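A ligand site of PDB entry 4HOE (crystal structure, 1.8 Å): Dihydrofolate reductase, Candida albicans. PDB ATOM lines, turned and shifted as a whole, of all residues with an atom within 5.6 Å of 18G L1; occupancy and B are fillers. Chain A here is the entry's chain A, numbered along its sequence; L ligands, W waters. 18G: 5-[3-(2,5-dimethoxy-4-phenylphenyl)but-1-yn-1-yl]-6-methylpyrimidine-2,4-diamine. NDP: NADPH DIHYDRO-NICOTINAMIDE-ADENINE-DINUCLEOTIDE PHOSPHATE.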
ATOM      1  N   ILE A   9     -25.929  -4.711  31.589  1.00  0.00           N
ATOM      2  CA  ILE A   9     -26.037  -3.832  30.413  1.00  0.00           C
ATOM      3  C   ILE A   9     -25.502  -4.589  29.184  1.00  0.00           C
ATOM      4  O   ILE A   9     -24.387  -5.118  29.218  1.00  0.00           O
ATOM      5  CB  ILE A   9     -25.374  -2.449  30.647  1.00  0.00           C
ATOM      6  CG1 ILE A   9     -25.674  -1.501  29.481  1.00  0.00           C
ATOM      7  CG2 ILE A   9     -23.885  -2.581  30.934  1.00  0.00           C
ATOM      8  CD1 ILE A   9     -25.379  -0.028  29.782  1.00  0.00           C
ATOM      9  N   VAL A  10     -26.308  -4.623  28.125  1.00  0.00           N
ATOM     10  CA  VAL A  10     -26.037  -5.451  26.945  1.00  0.00           C
ATOM     11  C   VAL A  10     -26.778  -4.894  25.719  1.00  0.00           C
ATOM     12  O   VAL A  10     -27.812  -4.240  25.858  1.00  0.00           O
ATOM     13  CB  VAL A  10     -26.397  -6.944  27.192  1.00  0.00           C
ATOM     14  CG1 VAL A  10     -27.891  -7.139  27.454  1.00  0.00           C
ATOM     15  CG2 VAL A  10     -25.925  -7.828  26.049  1.00  0.00           C
ATOM     16  N   ALA A  11     -26.229  -5.138  24.534  1.00  0.00           N
ATOM     17  CA  ALA A  11     -26.925  -4.849  23.278  1.00  0.00           C
ATOM     18  C   ALA A  11     -27.143  -6.152  22.531  1.00  0.00           C
ATOM     19  O   ALA A  11     -26.193  -6.905  22.302  1.00  0.00           O
ATOM     20  CB  ALA A  11     -26.110  -3.876  22.436  1.00  0.00           C
ATOM     21  N   MET A  25     -18.213  -8.493  18.270  1.00  0.00           N
ATOM     22  CA  MET A  25     -19.570  -7.979  18.110  1.00  0.00           C
ATOM     23  C   MET A  25     -19.938  -7.903  16.630  1.00  0.00           C
ATOM     24  O   MET A  25     -19.106  -7.501  15.806  1.00  0.00           O
ATOM     25  CB  MET A  25     -19.729  -6.616  18.789  1.00  0.00           C
ATOM     26  CG  MET A  25     -19.828  -6.710  20.295  1.00  0.00           C
ATOM     27  SD  MET A  25     -19.729  -5.105  21.080  1.00  0.00           S
ATOM     28  CE  MET A  25     -19.094  -5.586  22.677  1.00  0.00           C
ATOM     29  N   GLU A  32     -24.704   3.763  20.204  1.00  0.00           N
ATOM     30  CA  GLU A  32     -24.875   2.740  21.241  1.00  0.00           C
ATOM     31  C   GLU A  32     -23.631   2.663  22.137  1.00  0.00           C
ATOM     32  O   GLU A  32     -23.746   2.624  23.365  1.00  0.00           O
ATOM     33  CB  GLU A  32     -25.181   1.374  20.606  1.00  0.00           C
ATOM     34  CG  GLU A  32     -26.087   0.474  21.449  1.00  0.00           C
ATOM     35  CD  GLU A  32     -25.429  -0.022  22.726  1.00  0.00           C
ATOM     36  OE1 GLU A  32     -24.230  -0.371  22.664  1.00  0.00           O
ATOM     37  OE2 GLU A  32     -26.096  -0.074  23.788  1.00  0.00           O
ATOM     38  N   ILE A  33     -22.444   2.682  21.519  1.00  0.00           N
ATOM     39  CA  ILE A  33     -21.176   2.651  22.260  1.00  0.00           C
ATOM     40  C   ILE A  33     -21.058   3.872  23.187  1.00  0.00           C
ATOM     41  O   ILE A  33     -20.606   3.751  24.331  1.00  0.00           O
ATOM     42  CB  ILE A  33     -19.977   2.527  21.282  1.00  0.00           C
ATOM     43  CG1 ILE A  33     -19.988   1.137  20.631  1.00  0.00           C
ATOM     44  CG2 ILE A  33     -18.642   2.798  21.957  1.00  0.00           C
ATOM     45  CD1 ILE A  33     -19.140   1.016  19.380  1.00  0.00           C
ATOM     46  N   TYR A  35     -23.575   5.593  24.417  1.00  0.00           N
ATOM     47  CA  TYR A  35     -24.579   5.339  25.462  1.00  0.00           C
ATOM     48  C   TYR A  35     -23.994   4.452  26.556  1.00  0.00           C
ATOM     49  O   TYR A  35     -24.079   4.781  27.735  1.00  0.00           O
ATOM     50  CB  TYR A  35     -25.831   4.690  24.854  1.00  0.00           C
ATOM     51  CG  TYR A  35     -26.859   4.198  25.858  1.00  0.00           C
ATOM     52  CD1 TYR A  35     -27.817   5.059  26.382  1.00  0.00           C
ATOM     53  CD2 TYR A  35     -26.889   2.856  26.262  1.00  0.00           C
ATOM     54  CE1 TYR A  35     -28.773   4.614  27.277  1.00  0.00           C
ATOM     55  CE2 TYR A  35     -27.840   2.396  27.169  1.00  0.00           C
ATOM     56  CZ  TYR A  35     -28.785   3.283  27.670  1.00  0.00           C
ATOM     57  OH  TYR A  35     -29.750   2.858  28.561  1.00  0.00           O
ATOM     58  N   PHE A  36     -23.402   3.337  26.147  1.00  0.00           N
ATOM     59  CA  PHE A  36     -22.716   2.433  27.071  1.00  0.00           C
ATOM     60  C   PHE A  36     -21.700   3.184  27.937  1.00  0.00           C
ATOM     61  O   PHE A  36     -21.671   3.010  29.161  1.00  0.00           O
ATOM     62  CB  PHE A  36     -22.035   1.296  26.302  1.00  0.00           C
ATOM     63  CG  PHE A  36     -21.130   0.452  27.150  1.00  0.00           C
ATOM     64  CD1 PHE A  36     -21.660  -0.525  27.972  1.00  0.00           C
ATOM     65  CD2 PHE A  36     -19.758   0.656  27.142  1.00  0.00           C
ATOM     66  CE1 PHE A  36     -20.834  -1.305  28.769  1.00  0.00           C
ATOM     67  CE2 PHE A  36     -18.915  -0.115  27.943  1.00  0.00           C
ATOM     68  CZ  PHE A  36     -19.459  -1.106  28.754  1.00  0.00           C
ATOM     69  N   MET A  54     -16.667  -7.868  34.227  1.00  0.00           N
ATOM     70  CA  MET A  54     -16.654  -8.610  32.991  1.00  0.00           C
ATOM     71  C   MET A  54     -15.915  -9.924  33.122  1.00  0.00           C
ATOM     72  O   MET A  54     -15.108 -10.098  34.031  1.00  0.00           O
ATOM     73  CB  MET A  54     -16.036  -7.785  31.862  1.00  0.00           C
ATOM     74  CG  MET A  54     -14.529  -7.597  31.975  1.00  0.00           C
ATOM     75  SD  MET A  54     -13.939  -6.145  31.091  1.00  0.00           S
ATOM     76  CE  MET A  54     -14.020  -4.910  32.385  1.00  0.00           C
ATOM     77  N   THR A  58     -13.840 -11.227  27.659  1.00  0.00           N
ATOM     78  CA  THR A  58     -14.221  -9.868  27.248  1.00  0.00           C
ATOM     79  C   THR A  58     -13.106  -8.858  27.536  1.00  0.00           C
ATOM     80  O   THR A  58     -12.793  -8.028  26.694  1.00  0.00           O
ATOM     81  CB  THR A  58     -15.562  -9.452  27.871  1.00  0.00           C
ATOM     82  OG1 THR A  58     -16.600 -10.299  27.367  1.00  0.00           O
ATOM     83  CG2 THR A  58     -15.899  -7.981  27.550  1.00  0.00           C
ATOM     84  N   SER A  61     -10.436  -9.005  25.039  1.00  0.00           N
ATOM     85  CA  SER A  61     -10.873  -8.581  23.717  1.00  0.00           C
ATOM     86  C   SER A  61     -10.904  -7.057  23.576  1.00  0.00           C
ATOM     87  O   SER A  61     -11.052  -6.539  22.479  1.00  0.00           O
ATOM     88  CB  SER A  61     -12.216  -9.215  23.360  1.00  0.00           C
ATOM     89  OG  SER A  61     -12.049 -10.594  23.047  1.00  0.00           O
ATOM     90  N   ILE A  62     -10.783  -6.349  24.705  1.00  0.00           N
ATOM     91  CA  ILE A  62     -10.536  -4.902  24.674  1.00  0.00           C
ATOM     92  C   ILE A  62      -9.053  -4.709  24.346  1.00  0.00           C
ATOM     93  O   ILE A  62      -8.201  -5.257  25.040  1.00  0.00           O
ATOM     94  CB  ILE A  62     -10.846  -4.236  26.036  1.00  0.00           C
ATOM     95  CG1 ILE A  62     -12.252  -4.594  26.524  1.00  0.00           C
ATOM     96  CG2 ILE A  62     -10.684  -2.710  25.944  1.00  0.00           C
ATOM     97  CD1 ILE A  62     -12.479  -4.298  27.999  1.00  0.00           C
ATOM     98  N   PRO A  63      -8.735  -3.934  23.277  1.00  0.00           N
ATOM     99  CA  PRO A  63      -7.319  -3.744  22.958  1.00  0.00           C
ATOM    100  C   PRO A  63      -6.554  -3.187  24.168  1.00  0.00           C
ATOM    101  O   PRO A  63      -7.051  -2.287  24.851  1.00  0.00           O
ATOM    102  CB  PRO A  63      -7.356  -2.722  21.815  1.00  0.00           C
ATOM    103  CG  PRO A  63      -8.690  -2.959  21.183  1.00  0.00           C
ATOM    104  CD  PRO A  63      -9.608  -3.218  22.333  1.00  0.00           C
ATOM    105  N   PHE A  66      -6.603   0.323  25.531  1.00  0.00           N
ATOM    106  CA  PHE A  66      -7.880   0.932  25.864  1.00  0.00           C
ATOM    107  C   PHE A  66      -8.540   0.302  27.093  1.00  0.00           C
ATOM    108  O   PHE A  66      -9.691   0.586  27.405  1.00  0.00           O
ATOM    109  CB  PHE A  66      -8.810   0.903  24.647  1.00  0.00           C
ATOM    110  CG  PHE A  66      -8.321   1.745  23.500  1.00  0.00           C
ATOM    111  CD1 PHE A  66      -8.542   3.112  23.482  1.00  0.00           C
ATOM    112  CD2 PHE A  66      -7.644   1.153  22.434  1.00  0.00           C
ATOM    113  CE1 PHE A  66      -8.082   3.893  22.422  1.00  0.00           C
ATOM    114  CE2 PHE A  66      -7.178   1.921  21.372  1.00  0.00           C
ATOM    115  CZ  PHE A  66      -7.398   3.302  21.372  1.00  0.00           C
ATOM    116  N   LEU A  69     -11.217   0.342  31.122  1.00  0.00           N
ATOM    117  CA  LEU A  69     -12.157   1.370  30.648  1.00  0.00           C
ATOM    118  C   LEU A  69     -12.101   2.545  31.613  1.00  0.00           C
ATOM    119  O   LEU A  69     -12.254   2.377  32.827  1.00  0.00           O
ATOM    120  CB  LEU A  69     -13.570   0.805  30.531  1.00  0.00           C
ATOM    121  CG  LEU A  69     -13.794  -0.423  29.661  1.00  0.00           C
ATOM    122  CD1 LEU A  69     -15.258  -0.854  29.741  1.00  0.00           C
ATOM    123  CD2 LEU A  69     -13.397  -0.216  28.195  1.00  0.00           C
ATOM    124  N   ILE A 111     -22.753  -5.223  34.978  1.00  0.00           N
ATOM    125  CA  ILE A 111     -22.158  -6.370  34.288  1.00  0.00           C
ATOM    126  C   ILE A 111     -22.126  -6.070  32.790  1.00  0.00           C
ATOM    127  O   ILE A 111     -23.179  -5.856  32.184  1.00  0.00           O
ATOM    128  CB  ILE A 111     -22.955  -7.652  34.536  1.00  0.00           C
ATOM    129  CG1 ILE A 111     -22.981  -7.988  36.035  1.00  0.00           C
ATOM    130  CG2 ILE A 111     -22.381  -8.817  33.748  1.00  0.00           C
ATOM    131  CD1 ILE A 111     -24.154  -8.881  36.402  1.00  0.00           C
ATOM    132  N   ILE A 112     -20.938  -6.089  32.207  1.00  0.00           N
ATOM    133  CA  ILE A 112     -20.750  -5.620  30.838  1.00  0.00           C
ATOM    134  C   ILE A 112     -20.354  -6.694  29.827  1.00  0.00           C
ATOM    135  O   ILE A 112     -20.091  -6.397  28.659  1.00  0.00           O
ATOM    136  CB  ILE A 112     -19.772  -4.421  30.773  1.00  0.00           C
ATOM    137  CG1 ILE A 112     -18.334  -4.859  31.112  1.00  0.00           C
ATOM    138  CG2 ILE A 112     -20.226  -3.328  31.734  1.00  0.00           C
ATOM    139  CD1 ILE A 112     -17.279  -3.813  30.811  1.00  0.00           C
ATOM    140  N   GLY A 113     -20.339  -7.955  30.264  1.00  0.00           N
ATOM    141  CA  GLY A 113     -20.152  -9.084  29.330  1.00  0.00           C
ATOM    142  C   GLY A 113     -19.162 -10.108  29.837  1.00  0.00           C
ATOM    143  O   GLY A 113     -18.567  -9.892  30.890  1.00  0.00           O
ATOM    144  N   TYR A 118     -23.076 -13.132  31.373  1.00  0.00           N
ATOM    145  CA  TYR A 118     -24.494 -12.752  31.305  1.00  0.00           C
ATOM    146  C   TYR A 118     -25.417 -13.921  31.640  1.00  0.00           C
ATOM    147  O   TYR A 118     -26.360 -13.780  32.435  1.00  0.00           O
ATOM    148  CB  TYR A 118     -24.857 -12.292  29.895  1.00  0.00           C
ATOM    149  CG  TYR A 118     -24.354 -10.944  29.462  1.00  0.00           C
ATOM    150  CD1 TYR A 118     -24.429  -9.831  30.306  1.00  0.00           C
ATOM    151  CD2 TYR A 118     -23.888 -10.769  28.160  1.00  0.00           C
ATOM    152  CE1 TYR A 118     -23.990  -8.579  29.865  1.00  0.00           C
ATOM    153  CE2 TYR A 118     -23.456  -9.529  27.723  1.00  0.00           C
ATOM    154  CZ  TYR A 118     -23.519  -8.444  28.577  1.00  0.00           C
ATOM    155  OH  TYR A 118     -23.094  -7.227  28.113  1.00  0.00           O
ATOM    156  N   LEU A 131     -30.414  -3.472  31.472  1.00  0.00           N
ATOM    157  CA  LEU A 131     -30.402  -2.396  30.494  1.00  0.00           C
ATOM    158  C   LEU A 131     -30.104  -3.050  29.170  1.00  0.00           C
ATOM    159  O   LEU A 131     -28.938  -3.344  28.871  1.00  0.00           O
ATOM    160  CB  LEU A 131     -29.345  -1.355  30.850  1.00  0.00           C
ATOM    161  CG  LEU A 131     -29.624  -0.538  32.121  1.00  0.00           C
ATOM    162  CD1 LEU A 131     -28.347   0.163  32.545  1.00  0.00           C
ATOM    163  CD2 LEU A 131     -30.738   0.453  31.868  1.00  0.00           C
ATOM    164  N   THR A 133     -30.239  -2.966  25.091  1.00  0.00           N
ATOM    165  CA  THR A 133     -30.444  -2.238  23.851  1.00  0.00           C
ATOM    166  C   THR A 133     -30.987  -3.258  22.873  1.00  0.00           C
ATOM    167  O   THR A 133     -30.274  -4.183  22.466  1.00  0.00           O
ATOM    168  CB  THR A 133     -29.144  -1.598  23.319  1.00  0.00           C
ATOM    169  OG1 THR A 133     -28.622  -0.704  24.314  1.00  0.00           O
ATOM    170  CG2 THR A 133     -29.436  -0.796  22.045  1.00  0.00           C
HETATM  171  N2  18G L   1     -25.251  -1.801  25.750  1.00  0.00           N
HETATM  172  C14 18G L   1     -23.986  -2.225  25.713  1.00  0.00           C
HETATM  173  N1  18G L   1     -23.591  -3.112  26.659  1.00  0.00           N
HETATM  174  C13 18G L   1     -22.315  -3.551  26.598  1.00  0.00           C
HETATM  175  N   18G L   1     -21.952  -4.458  27.516  1.00  0.00           N
HETATM  176  N3  18G L   1     -23.203  -1.741  24.729  1.00  0.00           N
HETATM  177  C15 18G L   1     -21.931  -2.175  24.676  1.00  0.00           C
HETATM  178  C16 18G L   1     -21.078  -1.612  23.575  1.00  0.00           C
HETATM  179  C12 18G L   1     -21.413  -3.101  25.600  1.00  0.00           C
HETATM  180  C11 18G L   1     -20.066  -3.596  25.619  1.00  0.00           C
HETATM  181  C10 18G L   1     -18.973  -4.047  25.696  1.00  0.00           C
HETATM  182  C8  18G L   1     -17.622  -4.590  25.770  1.00  0.00           C
HETATM  183  C9  18G L   1     -17.161  -4.625  27.242  1.00  0.00           C
HETATM  184  C7  18G L   1     -16.612  -3.842  24.954  1.00  0.00           C
HETATM  185  C1  18G L   1     -15.564  -4.498  24.295  1.00  0.00           C
HETATM  186  O   18G L   1     -15.592  -5.859  24.385  1.00  0.00           O
HETATM  187  C   18G L   1     -14.425  -6.581  23.958  1.00  0.00           C
HETATM  188  C6  18G L   1     -16.667  -2.455  24.885  1.00  0.00           C
HETATM  189  C4  18G L   1     -15.699  -1.734  24.205  1.00  0.00           C
HETATM  190  O1  18G L   1     -15.712  -0.375  24.097  1.00  0.00           O
HETATM  191  C5  18G L   1     -16.780   0.331  24.729  1.00  0.00           C
HETATM  192  C3  18G L   1     -14.643  -2.388  23.561  1.00  0.00           C
HETATM  193  C2  18G L   1     -14.604  -3.782  23.613  1.00  0.00           C
HETATM  194  C17 18G L   1     -13.539  -1.649  22.892  1.00  0.00           C
HETATM  195  C22 18G L   1     -13.132  -1.980  21.595  1.00  0.00           C
HETATM  196  C21 18G L   1     -12.139  -1.255  20.960  1.00  0.00           C
HETATM  197  C20 18G L   1     -11.527  -0.198  21.595  1.00  0.00           C
HETATM  198  C19 18G L   1     -11.915   0.144  22.882  1.00  0.00           C
HETATM  199  C18 18G L   1     -12.902  -0.572  23.526  1.00  0.00           C
HETATM  200  PA  NDP L   2     -16.903 -13.921  28.763  1.00  0.00           P
HETATM  201  O1A NDP L   2     -18.271 -14.200  29.334  1.00  0.00           O
HETATM  202  O2A NDP L   2     -16.449 -12.501  28.566  1.00  0.00           O
HETATM  203  O5B NDP L   2     -15.759 -14.660  29.617  1.00  0.00           O
HETATM  204  C5B NDP L   2     -15.920 -16.026  30.002  1.00  0.00           C
HETATM  205  C4B NDP L   2     -14.850 -16.233  31.050  1.00  0.00           C
HETATM  206  O4B NDP L   2     -15.216 -15.563  32.258  1.00  0.00           O
HETATM  207  C3B NDP L   2     -14.654 -17.693  31.452  1.00  0.00           C
HETATM  208  O3B NDP L   2     -13.884 -18.428  30.515  1.00  0.00           O
HETATM  209  C2B NDP L   2     -14.011 -17.512  32.811  1.00  0.00           C
HETATM  210  O2B NDP L   2     -12.631 -17.151  32.698  1.00  0.00           O
HETATM  211  C1B NDP L   2     -14.777 -16.321  33.383  1.00  0.00           C
HETATM  212  N9A NDP L   2     -15.938 -16.798  34.180  1.00  0.00           N
HETATM  213  C8A NDP L   2     -17.145 -17.166  33.710  1.00  0.00           C
HETATM  214  N7A NDP L   2     -17.967 -17.553  34.718  1.00  0.00           N
HETATM  215  C5A NDP L   2     -17.285 -17.454  35.869  1.00  0.00           C
HETATM  216  C6A NDP L   2     -17.560 -17.699  37.313  1.00  0.00           C
HETATM  217  N6A NDP L   2     -18.753 -18.158  37.757  1.00  0.00           N
HETATM  218  N1A NDP L   2     -16.545 -17.454  38.173  1.00  0.00           N
HETATM  219  C2A NDP L   2     -15.336 -16.995  37.773  1.00  0.00           C
HETATM  220  N3A NDP L   2     -15.031 -16.743  36.476  1.00  0.00           N
HETATM  221  C4A NDP L   2     -15.950 -16.946  35.508  1.00  0.00           C
HETATM  222  O3  NDP L   2     -16.665 -14.705  27.366  1.00  0.00           O
HETATM  223  PN  NDP L   2     -17.709 -15.203  26.245  1.00  0.00           P
HETATM  224  O1N NDP L   2     -16.856 -15.767  25.116  1.00  0.00           O
HETATM  225  O2N NDP L   2     -18.778 -16.069  26.869  1.00  0.00           O
HETATM  226  O5D NDP L   2     -18.370 -13.840  25.680  1.00  0.00           O
HETATM  227  C5D NDP L   2     -17.733 -13.145  24.614  1.00  0.00           C
HETATM  228  C4D NDP L   2     -18.784 -12.730  23.586  1.00  0.00           C
HETATM  229  O4D NDP L   2     -19.700 -11.824  24.202  1.00  0.00           O
HETATM  230  C3D NDP L   2     -18.175 -12.003  22.387  1.00  0.00           C
HETATM  231  O3D NDP L   2     -18.711 -12.573  21.188  1.00  0.00           O
HETATM  232  C2D NDP L   2     -18.648 -10.579  22.511  1.00  0.00           C
HETATM  233  O2D NDP L   2     -18.929 -10.003  21.229  1.00  0.00           O
HETATM  234  C1D NDP L   2     -19.924 -10.710  23.333  1.00  0.00           C
HETATM  235  N1N NDP L   2     -20.259  -9.484  24.053  1.00  0.00           N
HETATM  236  C2N NDP L   2     -21.338  -8.830  23.620  1.00  0.00           C
HETATM  237  C3N NDP L   2     -21.750  -7.641  24.227  1.00  0.00           C
HETATM  238  C7N NDP L   2     -22.969  -6.946  23.693  1.00  0.00           C
HETATM  239  O7N NDP L   2     -23.474  -6.074  24.376  1.00  0.00           O
HETATM  240  N7N NDP L   2     -23.453  -7.298  22.496  1.00  0.00           N
HETATM  241  C4N NDP L   2     -21.025  -7.150  25.321  1.00  0.00           C
HETATM  242  C5N NDP L   2     -19.900  -7.852  25.755  1.00  0.00           C
HETATM  243  C6N NDP L   2     -19.534  -9.025  25.104  1.00  0.00           C
HETATM  244  P2B NDP L   2     -11.444 -18.240  32.705  1.00  0.00           P
HETATM  245  O1X NDP L   2     -11.592 -18.970  31.390  1.00  0.00           O
HETATM  246  O2X NDP L   2     -10.207 -17.413  32.784  1.00  0.00           O
HETATM  247  O3X NDP L   2     -11.735 -19.076  33.938  1.00  0.00           O
HETATM  248  O   HOH W   1     -17.900   3.195  25.112  1.00  0.00           O
HETATM  249  O   HOH W   2     -28.342  -1.153  27.087  1.00  0.00           O
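Residues that only touch 18G L1: Ala 11, Met 25, Phe 36, Thr 58, Ser 61, Ile 62, Pro 63, Phe 66 and Thr 133. Hydrophobic or aromatic side chains that line 18G L1: Ile 9, Met 25, Phe 36, Ile 62, Pro 63, Phe 66 and Ile 112. Within 4 Å of 18G L1: Ile 9, Val 10, Ala 11, Met 25, Glu 32, Phe 36, Thr 58, Ser 61, Ile 62, Pro 63, Phe 66, Ile 112, Tyr 118 and Thr 133. Along chain A the residues within 4 Å of 18G L1 span positions 9 to 133.
The side-chain carboxylate of Glu 32 is in hydrogen-bond range of the side-chain hydroxyl of Thr 133 (2.7 Å). OH of Tyr 118 lies within hydrogen-bond range of O of Ile 112, at 3.2 Å. The backbone NH (N) of Ile 9 lies within hydrogen-bond range of the backbone carbonyl oxygen (O) of Ile 111. The backbone NH (N) of Val 10 is in hydrogen-bond range of the backbone carbonyl oxygen (O) of Leu 131, 3.0 Å away. The side-chain hydroxyl of Tyr 118 sits at hydrogen-bond distance from the backbone carbonyl oxygen of Ile 9, 2.7 Å away. The backbone carbonyl oxygen of Val 10 is in hydrogen-bond range of the backbone NH of Thr 133.
O7N of NDP L2 lies within hydrogen-bond range of N of Ala 11 (2.9 Å). A nitrogen (N) of 18G L1 sits at hydrogen-bond distance from the side-chain hydroxyl (OH) of Tyr 118, at 3.1 Å. An oxygen (O2A) of NDP L2 sits at hydrogen-bond distance from the side-chain hydroxyl (OG1) of Thr 58, 2.5 Å away. N3 of 18G L1 sits at hydrogen-bond distance from OE1 of Glu 32. The backbone NH of Met 25 is in hydrogen-bond range of an oxygen (O2D) of NDP L2, 3.4 Å away. N of 18G L1 lies within hydrogen-bond range of O of Ile 112 (2.9 Å). O2A of NDP L2 lies within hydrogen-bond range of N of Thr 58 (3.0 Å). A nitrogen (N) of 18G L1 lies within hydrogen-bond range of the backbone carbonyl oxygen (O) of Ile 9. The backbone NH (N) of Val 10 lies close to a nitrogen (N1) of 18G L1, at 3.4 Å. The backbone carbonyl oxygen (O) of Ala 11 lies within hydrogen-bond range of a nitrogen (N7N) of NDP L2 (2.8 Å).
Water W2 lies within hydrogen-bond range of OG1 of Thr 133, O of Leu 131, O of Val 10 and N2 of 18G L1.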
